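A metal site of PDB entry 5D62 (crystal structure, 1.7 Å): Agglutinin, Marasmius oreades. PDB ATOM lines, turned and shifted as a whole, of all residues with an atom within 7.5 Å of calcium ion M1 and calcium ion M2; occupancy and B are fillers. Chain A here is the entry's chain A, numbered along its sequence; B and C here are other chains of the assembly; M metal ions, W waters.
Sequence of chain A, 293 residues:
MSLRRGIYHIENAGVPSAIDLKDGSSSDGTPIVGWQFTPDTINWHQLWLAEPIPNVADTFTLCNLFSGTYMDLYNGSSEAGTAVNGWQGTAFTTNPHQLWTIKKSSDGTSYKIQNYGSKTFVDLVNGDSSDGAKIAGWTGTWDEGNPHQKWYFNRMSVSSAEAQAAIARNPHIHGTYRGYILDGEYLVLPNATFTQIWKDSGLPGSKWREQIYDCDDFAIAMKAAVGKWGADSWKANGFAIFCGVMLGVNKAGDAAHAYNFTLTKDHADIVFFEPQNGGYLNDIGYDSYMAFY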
ATOM      1  N   TRP A 208     -10.512  30.726 -13.062  1.00  0.00           N
ATOM      2  CA  TRP A 208      -9.847  29.686 -13.755  1.00  0.00           C
ATOM      3  C   TRP A 208      -8.849  30.350 -14.754  1.00  0.00           C
ATOM      4  O   TRP A 208      -9.235  31.225 -15.560  1.00  0.00           O
ATOM      5  CB  TRP A 208     -10.833  28.805 -14.501  1.00  0.00           C
ATOM      6  CG  TRP A 208     -10.217  27.627 -15.219  1.00  0.00           C
ATOM      7  CD1 TRP A 208     -10.066  26.332 -14.713  1.00  0.00           C
ATOM      8  CD2 TRP A 208      -9.563  27.602 -16.488  1.00  0.00           C
ATOM      9  NE1 TRP A 208      -9.418  25.542 -15.617  1.00  0.00           N
ATOM     10  CE2 TRP A 208      -9.109  26.282 -16.710  1.00  0.00           C
ATOM     11  CE3 TRP A 208      -9.355  28.550 -17.484  1.00  0.00           C
ATOM     12  CZ2 TRP A 208      -8.462  25.892 -17.889  1.00  0.00           C
ATOM     13  CZ3 TRP A 208      -8.717  28.166 -18.654  1.00  0.00           C
ATOM     14  CH2 TRP A 208      -8.289  26.862 -18.847  1.00  0.00           C
ATOM     15  N   ARG A 209      -7.643  29.837 -14.729  1.00  0.00           N
ATOM     16  CA  ARG A 209      -6.548  30.301 -15.612  1.00  0.00           C
ATOM     17  C   ARG A 209      -5.742  29.064 -16.024  1.00  0.00           C
ATOM     18  O   ARG A 209      -5.359  28.246 -15.171  1.00  0.00           O
ATOM     19  CB  ARG A 209      -5.679  31.318 -14.942  1.00  0.00           C
ATOM     20  CG  ARG A 209      -6.371  32.634 -14.525  1.00  0.00           C
ATOM     21  CD  ARG A 209      -5.546  33.545 -13.588  1.00  0.00           C
ATOM     22  NE  ARG A 209      -4.286  33.912 -14.237  1.00  0.00           N
ATOM     23  CZ  ARG A 209      -3.204  34.404 -13.651  1.00  0.00           C
ATOM     24  NH1 ARG A 209      -3.231  34.770 -12.369  1.00  0.00           N
ATOM     25  NH2 ARG A 209      -2.115  34.550 -14.378  1.00  0.00           N
ATOM     26  N   GLU A 210      -5.498  28.959 -17.338  1.00  0.00           N
ATOM     27  CA  GLU A 210      -4.800  27.786 -17.909  1.00  0.00           C
ATOM     28  C   GLU A 210      -3.436  27.520 -17.224  1.00  0.00           C
ATOM     29  O   GLU A 210      -2.493  28.400 -17.139  1.00  0.00           O
ATOM     30  CB  GLU A 210      -4.640  27.999 -19.463  1.00  0.00           C
ATOM     31  CG  GLU A 210      -4.160  26.767 -20.201  1.00  0.00           C
ATOM     32  CD  GLU A 210      -4.091  26.985 -21.715  1.00  0.00           C
ATOM     33  OE1 GLU A 210      -4.507  28.037 -22.223  1.00  0.00           O
ATOM     34  OE2 GLU A 210      -3.604  26.091 -22.398  1.00  0.00           O
ATOM     35  N   GLN A 211      -3.323  26.311 -16.700  1.00  0.00           N
ATOM     36  CA  GLN A 211      -2.264  25.813 -15.870  1.00  0.00           C
ATOM     37  C   GLN A 211      -1.925  26.549 -14.569  1.00  0.00           C
ATOM     38  O   GLN A 211      -1.664  25.927 -13.549  1.00  0.00           O
ATOM     39  CB  GLN A 211      -0.964  25.619 -16.680  1.00  0.00           C
ATOM     40  CG  GLN A 211      -1.140  24.600 -17.827  1.00  0.00           C
ATOM     41  CD  GLN A 211       0.226  24.158 -18.415  1.00  0.00           C
ATOM     42  OE1 GLN A 211       1.155  23.814 -17.683  1.00  0.00           O
ATOM     43  NE2 GLN A 211       0.318  24.197 -19.757  1.00  0.00           N
ATOM     44  N   ILE A 212      -1.932  27.883 -14.575  1.00  0.00           N
ATOM     45  CA  ILE A 212      -1.428  28.659 -13.366  1.00  0.00           C
ATOM     46  C   ILE A 212      -2.484  28.686 -12.260  1.00  0.00           C
ATOM     47  O   ILE A 212      -2.107  28.933 -11.112  1.00  0.00           O
ATOM     48  CB  ILE A 212      -1.043  30.085 -13.856  1.00  0.00           C
ATOM     49  CG1 ILE A 212      -0.191  30.899 -12.834  1.00  0.00           C
ATOM     50  CG2 ILE A 212      -2.236  30.860 -14.292  1.00  0.00           C
ATOM     51  CD1 ILE A 212       1.151  30.225 -12.512  1.00  0.00           C
ATOM     52  N   TYR A 213      -3.770  28.564 -12.596  1.00  0.00           N
ATOM     53  CA  TYR A 213      -4.783  28.322 -11.540  1.00  0.00           C
ATOM     54  C   TYR A 213      -5.986  27.617 -12.151  1.00  0.00           C
ATOM     55  O   TYR A 213      -7.045  28.179 -12.428  1.00  0.00           O
ATOM     56  CB  TYR A 213      -5.137  29.630 -10.837  1.00  0.00           C
ATOM     57  CG  TYR A 213      -5.380  29.386  -9.341  1.00  0.00           C
ATOM     58  CD1 TYR A 213      -4.335  29.236  -8.463  1.00  0.00           C
ATOM     59  CD2 TYR A 213      -6.674  29.358  -8.834  1.00  0.00           C
ATOM     60  CE1 TYR A 213      -4.552  28.987  -7.129  1.00  0.00           C
ATOM     61  CE2 TYR A 213      -6.939  29.107  -7.513  1.00  0.00           C
ATOM     62  CZ  TYR A 213      -5.875  28.908  -6.639  1.00  0.00           C
ATOM     63  OH  TYR A 213      -6.050  28.671  -5.242  1.00  0.00           O
ATOM     64  N   ASP A 214      -5.754  26.341 -12.395  1.00  0.00           N
ATOM     65  CA  ASP A 214      -6.716  25.533 -13.099  1.00  0.00           C
ATOM     66  C   ASP A 214      -7.234  24.503 -12.087  1.00  0.00           C
ATOM     67  O   ASP A 214      -7.136  24.671 -10.864  1.00  0.00           O
ATOM     68  CB  ASP A 214      -6.159  24.916 -14.445  1.00  0.00           C
ATOM     69  CG  ASP A 214      -5.037  23.939 -14.279  1.00  0.00           C
ATOM     70  OD1 ASP A 214      -4.288  24.024 -13.247  1.00  0.00           O
ATOM     71  OD2 ASP A 214      -4.785  23.084 -15.236  1.00  0.00           O
ATOM     72  N   CYS A 215      -7.833  23.439 -12.586  1.00  0.00           N
ATOM     73  CA  CYS A 215      -8.713  22.615 -11.739  1.00  0.00           C
ATOM     74  C   CYS A 215      -7.871  22.046 -10.602  1.00  0.00           C
ATOM     75  O   CYS A 215      -8.355  21.957  -9.476  1.00  0.00           O
ATOM     76  CB  CYS A 215      -9.442  21.491 -12.552  1.00  0.00           C
ATOM     77  SG  CYS A 215      -8.299  20.435 -13.522  1.00  0.00           S
ATOM     78  N   ASP A 216      -6.659  21.580 -10.896  1.00  0.00           N
ATOM     79  CA  ASP A 216      -5.837  21.004  -9.879  1.00  0.00           C
ATOM     80  C   ASP A 216      -5.535  21.996  -8.757  1.00  0.00           C
ATOM     81  O   ASP A 216      -5.476  21.630  -7.551  1.00  0.00           O
ATOM     82  CB  ASP A 216      -4.567  20.377 -10.369  1.00  0.00           C
ATOM     83  CG  ASP A 216      -3.856  21.252 -11.393  1.00  0.00           C
ATOM     84  OD1 ASP A 216      -4.187  21.124 -12.602  1.00  0.00           O
ATOM     85  OD2 ASP A 216      -2.970  22.008 -10.980  1.00  0.00           O
ATOM     86  N   ASP A 217      -5.350  23.283  -9.083  1.00  0.00           N
ATOM     87  CA  ASP A 217      -5.092  24.290  -8.012  1.00  0.00           C
ATOM     88  C   ASP A 217      -6.334  24.508  -7.109  1.00  0.00           C
ATOM     89  O   ASP A 217      -6.167  24.682  -5.879  1.00  0.00           O
ATOM     90  CB  ASP A 217      -4.716  25.642  -8.666  1.00  0.00           C
ATOM     91  CG  ASP A 217      -3.438  25.493  -9.512  1.00  0.00           C
ATOM     92  OD1 ASP A 217      -2.401  25.477  -8.902  1.00  0.00           O
ATOM     93  OD2 ASP A 217      -3.478  25.307 -10.777  1.00  0.00           O
ATOM     94  N   PHE A 218      -7.548  24.583  -7.709  1.00  0.00           N
ATOM     95  CA  PHE A 218      -8.759  24.704  -6.931  1.00  0.00           C
ATOM     96  C   PHE A 218      -8.922  23.543  -5.985  1.00  0.00           C
ATOM     97  O   PHE A 218      -9.251  23.691  -4.829  1.00  0.00           O
ATOM     98  CB  PHE A 218      -9.995  24.794  -7.835  1.00  0.00           C
ATOM     99  CG  PHE A 218     -10.227  26.119  -8.466  1.00  0.00           C
ATOM    100  CD1 PHE A 218      -9.543  26.493  -9.684  1.00  0.00           C
ATOM    101  CD2 PHE A 218     -11.240  26.919  -8.043  1.00  0.00           C
ATOM    102  CE1 PHE A 218      -9.852  27.707 -10.307  1.00  0.00           C
ATOM    103  CE2 PHE A 218     -11.471  28.185  -8.583  1.00  0.00           C
ATOM    104  CZ  PHE A 218     -10.791  28.574  -9.710  1.00  0.00           C
ATOM    105  N   ALA A 258      -9.770  17.638 -11.990  1.00  0.00           N
ATOM    106  CA  ALA A 258      -9.401  17.531 -10.570  1.00  0.00           C
ATOM    107  C   ALA A 258     -10.541  18.180  -9.751  1.00  0.00           C
ATOM    108  O   ALA A 258     -11.078  19.231 -10.139  1.00  0.00           O
ATOM    109  CB  ALA A 258      -8.099  18.232 -10.308  1.00  0.00           C
ATOM    110  N   ILE B 181       0.978  13.731 -12.632  1.00  0.00           N
ATOM    111  CA  ILE B 181       1.302  14.978 -13.312  1.00  0.00           C
ATOM    112  C   ILE B 181       0.068  15.822 -13.405  1.00  0.00           C
ATOM    113  O   ILE B 181      -0.949  15.396 -13.919  1.00  0.00           O
ATOM    114  CB  ILE B 181       1.904  14.708 -14.690  1.00  0.00           C
ATOM    115  CG1 ILE B 181       3.253  14.015 -14.476  1.00  0.00           C
ATOM    116  CG2 ILE B 181       2.067  16.009 -15.499  1.00  0.00           C
ATOM    117  CD1 ILE B 181       3.938  13.595 -15.781  1.00  0.00           C
ATOM    118  N   LEU B 182       0.188  17.112 -13.003  1.00  0.00           N
ATOM    119  CA  LEU B 182      -0.969  17.982 -12.979  1.00  0.00           C
ATOM    120  C   LEU B 182      -1.015  19.064 -14.038  1.00  0.00           C
ATOM    121  O   LEU B 182      -2.100  19.621 -14.389  1.00  0.00           O
ATOM    122  CB  LEU B 182      -0.974  18.571 -11.568  1.00  0.00           C
ATOM    123  CG  LEU B 182      -1.086  17.666 -10.330  1.00  0.00           C
ATOM    124  CD1 LEU B 182      -1.008  18.458  -9.041  1.00  0.00           C
ATOM    125  CD2 LEU B 182      -2.401  16.985 -10.383  1.00  0.00           C
ATOM    126  N   ASP B 183       0.158  19.468 -14.516  1.00  0.00           N
ATOM    127  CA  ASP B 183       0.235  20.544 -15.522  1.00  0.00           C
ATOM    128  C   ASP B 183       1.320  20.163 -16.608  1.00  0.00           C
ATOM    129  O   ASP B 183       1.831  19.029 -16.605  1.00  0.00           O
ATOM    130  CB  ASP B 183       0.604  21.840 -14.818  1.00  0.00           C
ATOM    131  CG  ASP B 183      -0.517  22.369 -13.888  1.00  0.00           C
ATOM    132  OD1 ASP B 183      -1.633  22.621 -14.358  1.00  0.00           O
ATOM    133  OD2 ASP B 183      -0.245  22.599 -12.679  1.00  0.00           O
ATOM    134  N   GLY B 184       1.672  21.088 -17.477  1.00  0.00           N
ATOM    135  CA  GLY B 184       2.549  20.838 -18.655  1.00  0.00           C
ATOM    136  C   GLY B 184       3.879  21.502 -18.662  1.00  0.00           C
ATOM    137  O   GLY B 184       4.852  20.956 -19.234  1.00  0.00           O
ATOM    138  N   TYR B 186       6.499  24.226 -16.226  1.00  0.00           N
ATOM    139  CA  TYR B 186       6.670  24.751 -14.867  1.00  0.00           C
ATOM    140  C   TYR B 186       7.834  25.691 -14.699  1.00  0.00           C
ATOM    141  O   TYR B 186       8.982  25.363 -14.977  1.00  0.00           O
ATOM    142  CB  TYR B 186       6.920  23.570 -13.949  1.00  0.00           C
ATOM    143  CG  TYR B 186       5.848  22.504 -13.839  1.00  0.00           C
ATOM    144  CD1 TYR B 186       4.797  22.609 -12.893  1.00  0.00           C
ATOM    145  CD2 TYR B 186       5.868  21.375 -14.632  1.00  0.00           C
ATOM    146  CE1 TYR B 186       3.830  21.628 -12.769  1.00  0.00           C
ATOM    147  CE2 TYR B 186       4.934  20.339 -14.498  1.00  0.00           C
ATOM    148  CZ  TYR B 186       3.955  20.417 -13.541  1.00  0.00           C
ATOM    149  OH  TYR B 186       3.020  19.449 -13.386  1.00  0.00           O
ATOM    150  N   LYS B 223       2.409  23.215  -0.972  1.00  0.00           N
ATOM    151  CA  LYS B 223       2.052  23.152  -2.372  1.00  0.00           C
ATOM    152  C   LYS B 223       0.925  24.178  -2.710  1.00  0.00           C
ATOM    153  O   LYS B 223       0.962  24.847  -3.747  1.00  0.00           O
ATOM    154  CB  LYS B 223       1.575  21.770  -2.828  1.00  0.00           C
ATOM    155  CG  LYS B 223       1.279  21.754  -4.348  1.00  0.00           C
ATOM    156  CD  LYS B 223       1.414  20.355  -5.008  1.00  0.00           C
ATOM    157  CE  LYS B 223       1.122  20.391  -6.545  1.00  0.00           C
ATOM    158  NZ  LYS B 223       1.796  21.529  -7.321  1.00  0.00           N
ATOM    159  N   GLY B 227       1.072  27.411  -5.322  1.00  0.00           N
ATOM    160  CA  GLY B 227       0.031  27.628  -6.333  1.00  0.00           C
ATOM    161  C   GLY B 227      -0.625  29.018  -6.214  1.00  0.00           C
ATOM    162  O   GLY B 227      -0.826  29.690  -7.231  1.00  0.00           O
ATOM    163  N   PHE B 239       1.264  28.226 -17.954  1.00  0.00           N
ATOM    164  CA  PHE B 239       2.321  27.591 -17.245  1.00  0.00           C
ATOM    165  C   PHE B 239       1.903  27.466 -15.751  1.00  0.00           C
ATOM    166  O   PHE B 239       0.964  28.136 -15.308  1.00  0.00           O
ATOM    167  CB  PHE B 239       3.618  28.413 -17.325  1.00  0.00           C
ATOM    168  CG  PHE B 239       3.534  29.730 -16.558  1.00  0.00           C
ATOM    169  CD1 PHE B 239       2.802  30.791 -17.057  1.00  0.00           C
ATOM    170  CD2 PHE B 239       4.177  29.893 -15.354  1.00  0.00           C
ATOM    171  CE1 PHE B 239       2.652  32.001 -16.318  1.00  0.00           C
ATOM    172  CE2 PHE B 239       4.064  31.115 -14.630  1.00  0.00           C
ATOM    173  CZ  PHE B 239       3.287  32.111 -15.122  1.00  0.00           C
ATOM    174  N   ALA B 240       2.638  26.637 -15.020  1.00  0.00           N
ATOM    175  CA  ALA B 240       2.502  26.475 -13.581  1.00  0.00           C
ATOM    176  C   ALA B 240       3.813  26.767 -12.861  1.00  0.00           C
ATOM    177  O   ALA B 240       4.850  26.992 -13.505  1.00  0.00           O
ATOM    178  CB  ALA B 240       2.001  25.093 -13.235  1.00  0.00           C
ATOM    179  N   ILE B 241       3.827  26.746 -11.526  1.00  0.00           N
ATOM    180  CA  ILE B 241       5.047  26.860 -10.751  1.00  0.00           C
ATOM    181  C   ILE B 241       5.449  25.474 -10.180  1.00  0.00           C
ATOM    182  O   ILE B 241       4.572  24.779  -9.640  1.00  0.00           O
ATOM    183  CB  ILE B 241       4.832  27.707  -9.556  1.00  0.00           C
ATOM    184  CG1 ILE B 241       4.103  29.041  -9.976  1.00  0.00           C
ATOM    185  CG2 ILE B 241       6.133  28.029  -8.832  1.00  0.00           C
ATOM    186  CD1 ILE B 241       4.723  29.897 -11.062  1.00  0.00           C
ATOM    187  N   TYR B 293       2.561  16.756  -8.669  1.00  0.00           N
ATOM    188  CA  TYR B 293       3.285  18.005  -8.991  1.00  0.00           C
ATOM    189  C   TYR B 293       2.696  18.518 -10.301  1.00  0.00           C
ATOM    190  O   TYR B 293       2.679  19.705 -10.533  1.00  0.00           O
ATOM    191  CB  TYR B 293       4.790  17.748  -9.140  1.00  0.00           C
ATOM    192  CG  TYR B 293       5.193  16.628 -10.090  1.00  0.00           C
ATOM    193  CD1 TYR B 293       5.281  15.273  -9.670  1.00  0.00           C
ATOM    194  CD2 TYR B 293       5.522  16.936 -11.397  1.00  0.00           C
ATOM    195  CE1 TYR B 293       5.672  14.278 -10.559  1.00  0.00           C
ATOM    196  CE2 TYR B 293       5.897  15.914 -12.307  1.00  0.00           C
ATOM    197  CZ  TYR B 293       6.013  14.620 -11.866  1.00  0.00           C
ATOM    198  OH  TYR B 293       6.432  13.614 -12.797  1.00  0.00           O
ATOM    199  OXT TYR B 293       2.156  17.735 -11.138  1.00  0.00           O
ATOM    200  N   ASP C   4     -10.961  22.750 -17.384  1.00  0.00           N
ATOM    201  CA  ASP C   4     -10.018  21.710 -17.229  1.00  0.00           C
ATOM    202  C   ASP C   4      -9.196  21.690 -15.897  1.00  0.00           C
ATOM    203  O   ASP C   4      -8.606  22.723 -15.535  1.00  0.00           O
ATOM    204  CB  ASP C   4      -9.022  21.873 -18.390  1.00  0.00           C
ATOM    205  CG  ASP C   4      -8.312  20.626 -18.705  1.00  0.00           C
ATOM    206  OD1 ASP C   4      -8.642  19.607 -18.074  1.00  0.00           O
ATOM    207  OD2 ASP C   4      -7.438  20.682 -19.597  1.00  0.00           O
ATOM    208  C1  CF0 C   5      -9.088  20.478 -15.027  1.00  0.00           C
HETATM  209 CA    CA M   1      -2.193  23.956 -12.247  1.00  0.00          CA
HETATM  210 CA    CA M   2      -3.513  21.256 -14.813  1.00  0.00          CA
HETATM  211  O   HOH W   1      -2.955  21.165 -17.207  1.00  0.00           O
HETATM  212  O   HOH W   2      -0.646  24.500 -10.566  1.00  0.00           O
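Calcium ion M2 is bound by O of Leu 182 of chain B (2.2 Å), OD2 of Asp 214 (2.3 Å), OD1 of Asp 216 (2.3 Å), OD1 of Asp 183 of chain B (2.4 Å) and water W1 (2.5 Å).
OD1 of Asp 214 binds calcium ion M1.
Water W2 binds calcium ion M1.
OD2 of Asp 217 binds calcium ion M1 (2.4 Å).
OD2 of Asp 183 of chain B binds calcium ion M1 (2.4 Å).
Calcium ion M1 is bound by O of Gln 211 (2.4 Å).
Calcium ion M1 is bound by OD2 of Asp 216.
OD1 of Asp 183 of chain B binds calcium ion M1.
Calcium ion M1 has seven donor atoms within binding distance.
Within 4 Å of calcium ion M1: Gln 211, Asp 214, Asp 216, Asp 217 and Asp 183 of chain B.
The nearest printed residue that does not touch calcium ion M1 is Ala 240 of chain B (4.5 Å).
Four residues have an atom within 4 Å of calcium ion M2: Asp 214, Asp 216, Leu 182 of chain B and Asp 183 of chain B.
N of Asp 214 sits at hydrogen-bond distance from O of Arg 209 (3.4 Å).
The backbone NH (N) of Asp 183 of chain B lies within hydrogen-bond range of the side-chain hydroxyl (OH) of Tyr 186 of chain B (3.1 Å).
OE1 of Gln 211 sits at hydrogen-bond distance from N of Gly 184 of chain B (2.8 Å).
The backbone NH (N) of Leu 182 of chain B sits at hydrogen-bond distance from the chain-end carboxylate (OXT) of Tyr 293 of chain B (2.8 Å).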
